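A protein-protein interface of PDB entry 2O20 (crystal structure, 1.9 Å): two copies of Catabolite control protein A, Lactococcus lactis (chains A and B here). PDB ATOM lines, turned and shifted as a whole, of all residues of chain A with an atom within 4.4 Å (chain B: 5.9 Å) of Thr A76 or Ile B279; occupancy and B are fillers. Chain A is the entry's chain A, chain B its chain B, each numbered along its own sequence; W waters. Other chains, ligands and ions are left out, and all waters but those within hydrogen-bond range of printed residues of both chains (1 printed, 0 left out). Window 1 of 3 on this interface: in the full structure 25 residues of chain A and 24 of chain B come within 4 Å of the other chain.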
ATOM      1  N   THR A  74     -23.916   4.556 -34.448  1.00  0.00           N
ATOM      2  CA  THR A  74     -24.746   3.489 -33.875  1.00  0.00           C
ATOM      3  C   THR A  74     -24.659   3.352 -32.338  1.00  0.00           C
ATOM      4  O   THR A  74     -25.440   2.583 -31.761  1.00  0.00           O
ATOM      5  CB  THR A  74     -24.532   2.103 -34.561  1.00  0.00           C
ATOM      6  OG1 THR A  74     -23.167   1.662 -34.407  1.00  0.00           O
ATOM      7  CG2 THR A  74     -24.907   2.158 -36.023  1.00  0.00           C
ATOM      8  N   SER A  75     -23.759   4.088 -31.688  1.00  0.00           N
ATOM      9  CA  SER A  75     -23.669   4.125 -30.221  1.00  0.00           C
ATOM     10  C   SER A  75     -24.766   5.014 -29.674  1.00  0.00           C
ATOM     11  O   SER A  75     -24.922   6.177 -30.111  1.00  0.00           O
ATOM     12  CB  SER A  75     -22.326   4.682 -29.742  1.00  0.00           C
ATOM     13  OG  SER A  75     -22.354   5.028 -28.378  1.00  0.00           O
ATOM     14  N   THR A  76     -25.513   4.494 -28.722  1.00  0.00           N
ATOM     15  CA  THR A  76     -26.539   5.306 -28.070  1.00  0.00           C
ATOM     16  C   THR A  76     -25.912   6.414 -27.192  1.00  0.00           C
ATOM     17  O   THR A  76     -26.556   7.467 -26.958  1.00  0.00           O
ATOM     18  CB  THR A  76     -27.622   4.512 -27.278  1.00  0.00           C
ATOM     19  OG1 THR A  76     -27.083   3.863 -26.110  1.00  0.00           O
ATOM     20  CG2 THR A  76     -28.390   3.498 -28.131  1.00  0.00           C
ATOM     21  N   TYR A  77     -24.691   6.175 -26.712  1.00  0.00           N
ATOM     22  CA  TYR A  77     -23.919   7.195 -25.965  1.00  0.00           C
ATOM     23  C   TYR A  77     -23.544   8.369 -26.873  1.00  0.00           C
ATOM     24  O   TYR A  77     -23.936   9.496 -26.632  1.00  0.00           O
ATOM     25  CB  TYR A  77     -22.676   6.580 -25.298  1.00  0.00           C
ATOM     26  CG  TYR A  77     -21.886   7.565 -24.429  1.00  0.00           C
ATOM     27  CD1 TYR A  77     -22.242   7.799 -23.107  1.00  0.00           C
ATOM     28  CD2 TYR A  77     -20.804   8.266 -24.938  1.00  0.00           C
ATOM     29  CE1 TYR A  77     -21.515   8.736 -22.293  1.00  0.00           C
ATOM     30  CE2 TYR A  77     -20.080   9.183 -24.143  1.00  0.00           C
ATOM     31  CZ  TYR A  77     -20.440   9.409 -22.827  1.00  0.00           C
ATOM     32  OH  TYR A  77     -19.740  10.317 -22.054  1.00  0.00           O
ATOM     33  N   PHE A  78     -22.789   8.089 -27.934  1.00  0.00           N
ATOM     34  CA  PHE A  78     -22.247   9.135 -28.807  1.00  0.00           C
ATOM     35  C   PHE A  78     -23.296   9.811 -29.680  1.00  0.00           C
ATOM     36  O   PHE A  78     -23.194  11.005 -29.924  1.00  0.00           O
ATOM     37  CB  PHE A  78     -21.069   8.596 -29.661  1.00  0.00           C
ATOM     38  CG  PHE A  78     -19.879   8.242 -28.847  1.00  0.00           C
ATOM     39  CD1 PHE A  78     -19.163   9.222 -28.172  1.00  0.00           C
ATOM     40  CD2 PHE A  78     -19.488   6.906 -28.727  1.00  0.00           C
ATOM     41  CE1 PHE A  78     -18.087   8.880 -27.366  1.00  0.00           C
ATOM     42  CE2 PHE A  78     -18.421   6.554 -27.913  1.00  0.00           C
ATOM     43  CZ  PHE A  78     -17.707   7.557 -27.246  1.00  0.00           C
ATOM     44  N   ALA A  79     -24.320   9.075 -30.121  1.00  0.00           N
ATOM     45  CA  ALA A  79     -25.410   9.641 -30.939  1.00  0.00           C
ATOM     46  C   ALA A  79     -26.237  10.708 -30.169  1.00  0.00           C
ATOM     47  O   ALA A  79     -26.683  11.713 -30.739  1.00  0.00           O
ATOM     48  CB  ALA A  79     -26.319   8.518 -31.446  1.00  0.00           C
ATOM     49  N   ALA A  80     -26.429  10.469 -28.878  1.00  0.00           N
ATOM     50  CA  ALA A  80     -27.195  11.369 -27.992  1.00  0.00           C
ATOM     51  C   ALA A  80     -26.487  12.718 -27.875  1.00  0.00           C
ATOM     52  O   ALA A  80     -27.128  13.797 -27.983  1.00  0.00           O
ATOM     53  CB  ALA A  80     -27.375  10.732 -26.575  1.00  0.00           C
ATOM     54  N   SER A 277     -27.203   6.292 -20.725  1.00  0.00           N
ATOM     55  CA  SER A 277     -27.662   6.201 -22.092  1.00  0.00           C
ATOM     56  C   SER A 277     -28.925   5.314 -22.136  1.00  0.00           C
ATOM     57  O   SER A 277     -29.221   4.596 -21.170  1.00  0.00           O
ATOM     58  CB  SER A 277     -26.576   5.645 -23.010  1.00  0.00           C
ATOM     59  OG  SER A 277     -26.268   4.301 -22.673  1.00  0.00           O
ATOM     60  N   PRO A 278     -29.696   5.395 -23.239  1.00  0.00           N
ATOM     61  CA  PRO A 278     -30.993   4.703 -23.290  1.00  0.00           C
ATOM     62  C   PRO A 278     -30.983   3.223 -22.890  1.00  0.00           C
ATOM     63  O   PRO A 278     -31.975   2.741 -22.301  1.00  0.00           O
ATOM     64  CB  PRO A 278     -31.391   4.842 -24.759  1.00  0.00           C
ATOM     65  CG  PRO A 278     -30.781   6.113 -25.183  1.00  0.00           C
ATOM     66  CD  PRO A 278     -29.487   6.235 -24.426  1.00  0.00           C
ATOM     67  N   ILE A 279     -29.893   2.519 -23.231  1.00  0.00           N
ATOM     68  CA  ILE A 279     -29.816   1.078 -23.020  1.00  0.00           C
ATOM     69  C   ILE A 279     -29.884   0.644 -21.543  1.00  0.00           C
ATOM     70  O   ILE A 279     -30.156  -0.527 -21.264  1.00  0.00           O
ATOM     71  CB  ILE A 279     -28.587   0.436 -23.755  1.00  0.00           C
ATOM     72  CG1 ILE A 279     -27.237   0.904 -23.144  1.00  0.00           C
ATOM     73  CG2 ILE A 279     -28.668   0.703 -25.257  1.00  0.00           C
ATOM     74  CD1 ILE A 279     -25.976   0.207 -23.674  1.00  0.00           C
ATOM     75  N   TYR A 282     -33.206  -0.926 -20.786  1.00  0.00           N
ATOM     76  CA  TYR A 282     -33.667  -2.017 -21.655  1.00  0.00           C
ATOM     77  C   TYR A 282     -33.486  -3.423 -21.042  1.00  0.00           C
ATOM     78  O   TYR A 282     -33.984  -4.413 -21.594  1.00  0.00           O
ATOM     79  CB  TYR A 282     -32.933  -1.959 -23.003  1.00  0.00           C
ATOM     80  CG  TYR A 282     -33.180  -0.727 -23.839  1.00  0.00           C
ATOM     81  CD1 TYR A 282     -34.153   0.219 -23.501  1.00  0.00           C
ATOM     82  CD2 TYR A 282     -32.473  -0.535 -25.028  1.00  0.00           C
ATOM     83  CE1 TYR A 282     -34.381   1.345 -24.301  1.00  0.00           C
ATOM     84  CE2 TYR A 282     -32.681   0.599 -25.815  1.00  0.00           C
ATOM     85  CZ  TYR A 282     -33.630   1.527 -25.462  1.00  0.00           C
ATOM     86  OH  TYR A 282     -33.851   2.656 -26.235  1.00  0.00           O
ATOM     87  N   THR B  74     -30.361   9.447 -33.333  1.00  0.00           N
ATOM     88  CA  THR B  74     -30.506   8.600 -32.139  1.00  0.00           C
ATOM     89  C   THR B  74     -31.377   7.344 -32.319  1.00  0.00           C
ATOM     90  O   THR B  74     -31.529   6.566 -31.383  1.00  0.00           O
ATOM     91  CB  THR B  74     -31.083   9.402 -30.947  1.00  0.00           C
ATOM     92  OG1 THR B  74     -32.390   9.850 -31.298  1.00  0.00           O
ATOM     93  CG2 THR B  74     -30.192  10.576 -30.597  1.00  0.00           C
ATOM     94  N   THR B  76     -30.986   3.799 -33.667  1.00  0.00           N
ATOM     95  CA  THR B  76     -29.896   2.958 -34.136  1.00  0.00           C
ATOM     96  C   THR B  76     -30.272   2.236 -35.431  1.00  0.00           C
ATOM     97  O   THR B  76     -29.382   1.828 -36.155  1.00  0.00           O
ATOM     98  CB  THR B  76     -29.402   1.917 -33.103  1.00  0.00           C
ATOM     99  OG1 THR B  76     -30.456   1.027 -32.729  1.00  0.00           O
ATOM    100  CG2 THR B  76     -28.828   2.586 -31.895  1.00  0.00           C
ATOM    101  N   ASP B 248     -38.238  -1.759 -33.433  1.00  0.00           N
ATOM    102  CA  ASP B 248     -37.487  -2.290 -32.302  1.00  0.00           C
ATOM    103  C   ASP B 248     -37.647  -1.467 -31.021  1.00  0.00           C
ATOM    104  O   ASP B 248     -37.740  -2.039 -29.947  1.00  0.00           O
ATOM    105  CB  ASP B 248     -35.978  -2.354 -32.647  1.00  0.00           C
ATOM    106  CG  ASP B 248     -35.650  -3.365 -33.741  1.00  0.00           C
ATOM    107  OD1 ASP B 248     -36.317  -4.433 -33.898  1.00  0.00           O
ATOM    108  OD2 ASP B 248     -34.693  -3.053 -34.490  1.00  0.00           O
ATOM    109  N   THR B 249     -37.640  -0.139 -31.118  1.00  0.00           N
ATOM    110  CA  THR B 249     -37.761   0.713 -29.937  1.00  0.00           C
ATOM    111  C   THR B 249     -39.092   0.468 -29.216  1.00  0.00           C
ATOM    112  O   THR B 249     -39.138   0.405 -28.003  1.00  0.00           O
ATOM    113  CB  THR B 249     -37.697   2.200 -30.278  1.00  0.00           C
ATOM    114  OG1 THR B 249     -38.526   2.434 -31.430  1.00  0.00           O
ATOM    115  CG2 THR B 249     -36.267   2.644 -30.548  1.00  0.00           C
ATOM    116  N   VAL B 252     -38.949  -3.100 -27.500  1.00  0.00           N
ATOM    117  CA  VAL B 252     -38.144  -3.038 -26.300  1.00  0.00           C
ATOM    118  C   VAL B 252     -38.942  -2.374 -25.167  1.00  0.00           C
ATOM    119  O   VAL B 252     -38.845  -2.818 -24.013  1.00  0.00           O
ATOM    120  CB  VAL B 252     -36.790  -2.321 -26.521  1.00  0.00           C
ATOM    121  CG1 VAL B 252     -36.008  -2.201 -25.233  1.00  0.00           C
ATOM    122  CG2 VAL B 252     -35.930  -3.067 -27.545  1.00  0.00           C
ATOM    123  N   SER B 277     -32.183  -4.074 -34.949  1.00  0.00           N
ATOM    124  CA  SER B 277     -31.251  -2.955 -34.897  1.00  0.00           C
ATOM    125  C   SER B 277     -30.291  -3.080 -33.700  1.00  0.00           C
ATOM    126  O   SER B 277     -30.541  -3.885 -32.780  1.00  0.00           O
ATOM    127  CB  SER B 277     -32.034  -1.622 -34.854  1.00  0.00           C
ATOM    128  OG  SER B 277     -32.765  -1.460 -33.651  1.00  0.00           O
ATOM    129  N   PRO B 278     -29.200  -2.293 -33.699  1.00  0.00           N
ATOM    130  CA  PRO B 278     -28.217  -2.416 -32.624  1.00  0.00           C
ATOM    131  C   PRO B 278     -28.705  -2.390 -31.173  1.00  0.00           C
ATOM    132  O   PRO B 278     -28.172  -3.155 -30.372  1.00  0.00           O
ATOM    133  CB  PRO B 278     -27.195  -1.313 -32.940  1.00  0.00           C
ATOM    134  CG  PRO B 278     -27.307  -1.139 -34.433  1.00  0.00           C
ATOM    135  CD  PRO B 278     -28.736  -1.375 -34.764  1.00  0.00           C
ATOM    136  N   ILE B 279     -29.743  -1.620 -30.842  1.00  0.00           N
ATOM    137  CA  ILE B 279     -30.238  -1.629 -29.452  1.00  0.00           C
ATOM    138  C   ILE B 279     -30.749  -2.978 -28.937  1.00  0.00           C
ATOM    139  O   ILE B 279     -30.744  -3.200 -27.720  1.00  0.00           O
ATOM    140  CB  ILE B 279     -31.357  -0.575 -29.182  1.00  0.00           C
ATOM    141  CG1 ILE B 279     -32.557  -0.714 -30.142  1.00  0.00           C
ATOM    142  CG2 ILE B 279     -30.753   0.788 -29.144  1.00  0.00           C
ATOM    143  CD1 ILE B 279     -33.872  -0.098 -29.589  1.00  0.00           C
ATOM    144  N   THR B 280     -31.236  -3.831 -29.847  1.00  0.00           N
ATOM    145  CA  THR B 280     -31.817  -5.131 -29.469  1.00  0.00           C
ATOM    146  C   THR B 280     -30.787  -6.057 -28.782  1.00  0.00           C
ATOM    147  O   THR B 280     -31.164  -6.928 -28.003  1.00  0.00           O
ATOM    148  CB  THR B 280     -32.457  -5.858 -30.691  1.00  0.00           C
ATOM    149  OG1 THR B 280     -31.414  -6.321 -31.541  1.00  0.00           O
ATOM    150  CG2 THR B 280     -33.357  -4.912 -31.470  1.00  0.00           C
ATOM    151  N   GLN B 281     -29.492  -5.869 -29.043  1.00  0.00           N
ATOM    152  CA  GLN B 281     -28.448  -6.626 -28.344  1.00  0.00           C
ATOM    153  C   GLN B 281     -28.462  -6.416 -26.817  1.00  0.00           C
ATOM    154  O   GLN B 281     -28.034  -7.296 -26.064  1.00  0.00           O
ATOM    155  CB  GLN B 281     -27.043  -6.296 -28.893  1.00  0.00           C
ATOM    156  CG  GLN B 281     -25.893  -7.023 -28.145  1.00  0.00           C
ATOM    157  CD  GLN B 281     -24.510  -6.767 -28.728  1.00  0.00           C
ATOM    158  OE1 GLN B 281     -24.195  -5.644 -29.110  1.00  0.00           O
ATOM    159  NE2 GLN B 281     -23.670  -7.810 -28.779  1.00  0.00           N
ATOM    160  N   TYR B 282     -28.983  -5.272 -26.381  1.00  0.00           N
ATOM    161  CA  TYR B 282     -28.860  -4.843 -24.999  1.00  0.00           C
ATOM    162  C   TYR B 282     -30.132  -5.119 -24.191  1.00  0.00           C
ATOM    163  O   TYR B 282     -30.269  -4.660 -23.075  1.00  0.00           O
ATOM    164  CB  TYR B 282     -28.477  -3.356 -24.960  1.00  0.00           C
ATOM    165  CG  TYR B 282     -27.132  -3.106 -25.615  1.00  0.00           C
ATOM    166  CD1 TYR B 282     -25.962  -3.501 -24.991  1.00  0.00           C
ATOM    167  CD2 TYR B 282     -27.048  -2.522 -26.878  1.00  0.00           C
ATOM    168  CE1 TYR B 282     -24.733  -3.289 -25.580  1.00  0.00           C
ATOM    169  CE2 TYR B 282     -25.834  -2.314 -27.496  1.00  0.00           C
ATOM    170  CZ  TYR B 282     -24.675  -2.712 -26.843  1.00  0.00           C
ATOM    171  OH  TYR B 282     -23.476  -2.529 -27.445  1.00  0.00           O
ATOM    172  N   THR B 283     -31.068  -5.881 -24.733  1.00  0.00           N
ATOM    173  CA  THR B 283     -32.244  -6.230 -23.943  1.00  0.00           C
ATOM    174  C   THR B 283     -31.949  -7.400 -22.993  1.00  0.00           C
ATOM    175  O   THR B 283     -31.163  -8.297 -23.293  1.00  0.00           O
ATOM    176  CB  THR B 283     -33.470  -6.536 -24.807  1.00  0.00           C
ATOM    177  OG1 THR B 283     -33.272  -7.773 -25.504  1.00  0.00           O
ATOM    178  CG2 THR B 283     -33.705  -5.403 -25.790  1.00  0.00           C
HETATM  179  O   HOH W   1     -36.546  -4.667 -22.711  1.00  0.00           O
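The backbone carbonyl oxygen (O) of Thr B280 lies within hydrogen-bond range of the side-chain hydroxyl (OG1) of Thr B283, 3.4 Å away.
The side-chain hydroxyl of Thr B76 lies within hydrogen-bond range of the backbone NH of Ile B279 (3.3 Å).
Thr B76 touches Thr A74.
CG2 of Thr B76 touches CG2 of Thr A76 (3.9 Å).
Ile B279 touches Thr A76 (CG2 to CG2, 3.7 Å).
Ala A79 touches Thr B74.
CD1 of Ile A279 touches CD1 of Tyr B282, at 3.9 Å.
CG1 of Val B252 touches CG of Tyr A282, at 3.5 Å.
Tyr A282 touches Ile B279 (CE2 to CB, 3.8 Å).
Tyr B282 touches Tyr A282.
Tyr A282 touches Thr B283 (O to CA, 3.4 Å).
Thr A76 touches two residues of chain B.
Of chain A, only Thr A76 and Tyr A282 come within 4 Å of Ile B279.
Of the printed residues of chain A, Thr B74 touches Ala A79.
Printed residues of chain A within 4 Å of Thr B283: Tyr A282.
The nearest printed residue of chain A that does not touch Ile B279 is Ile A279 (4.4 Å).
The nearest printed residue of chain A that does not touch Thr B76 is Ser A75 (5.2 Å).
Hydrophobic or aromatic side chains of chain B that line the printed part of chain A: Val B252, Ile B279 and Tyr B282.
Of the 11 printed residues of chain A, 5 touch a printed residue of chain B.
Hydrophobic or aromatic side chains of chain A within 4 Å of the printed part of chain B: Ile A279 and Tyr A282.
Thr A76 touches its own counterpart, Thr B76.
Thr A76 touches Ile B279, but with the chains exchanged Ile A279 does not touch Thr B76 (6.9 Å).
Ile A279 touches Tyr B282, and with the chains exchanged Tyr A282 touches Ile B279.
Tyr A282 touches its own counterpart, Tyr B282.
6 positions are printed for both chains.
Of the 9 pairs that touch across the chains among the printed residues, 4 have their exchanged pair printed and touching as well.
Water W1 bridges the backbone carbonyl oxygen (O) of Tyr A282 (2.8 Å) and the backbone carbonyl oxygen (O) of Val B252 (3.2 Å).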
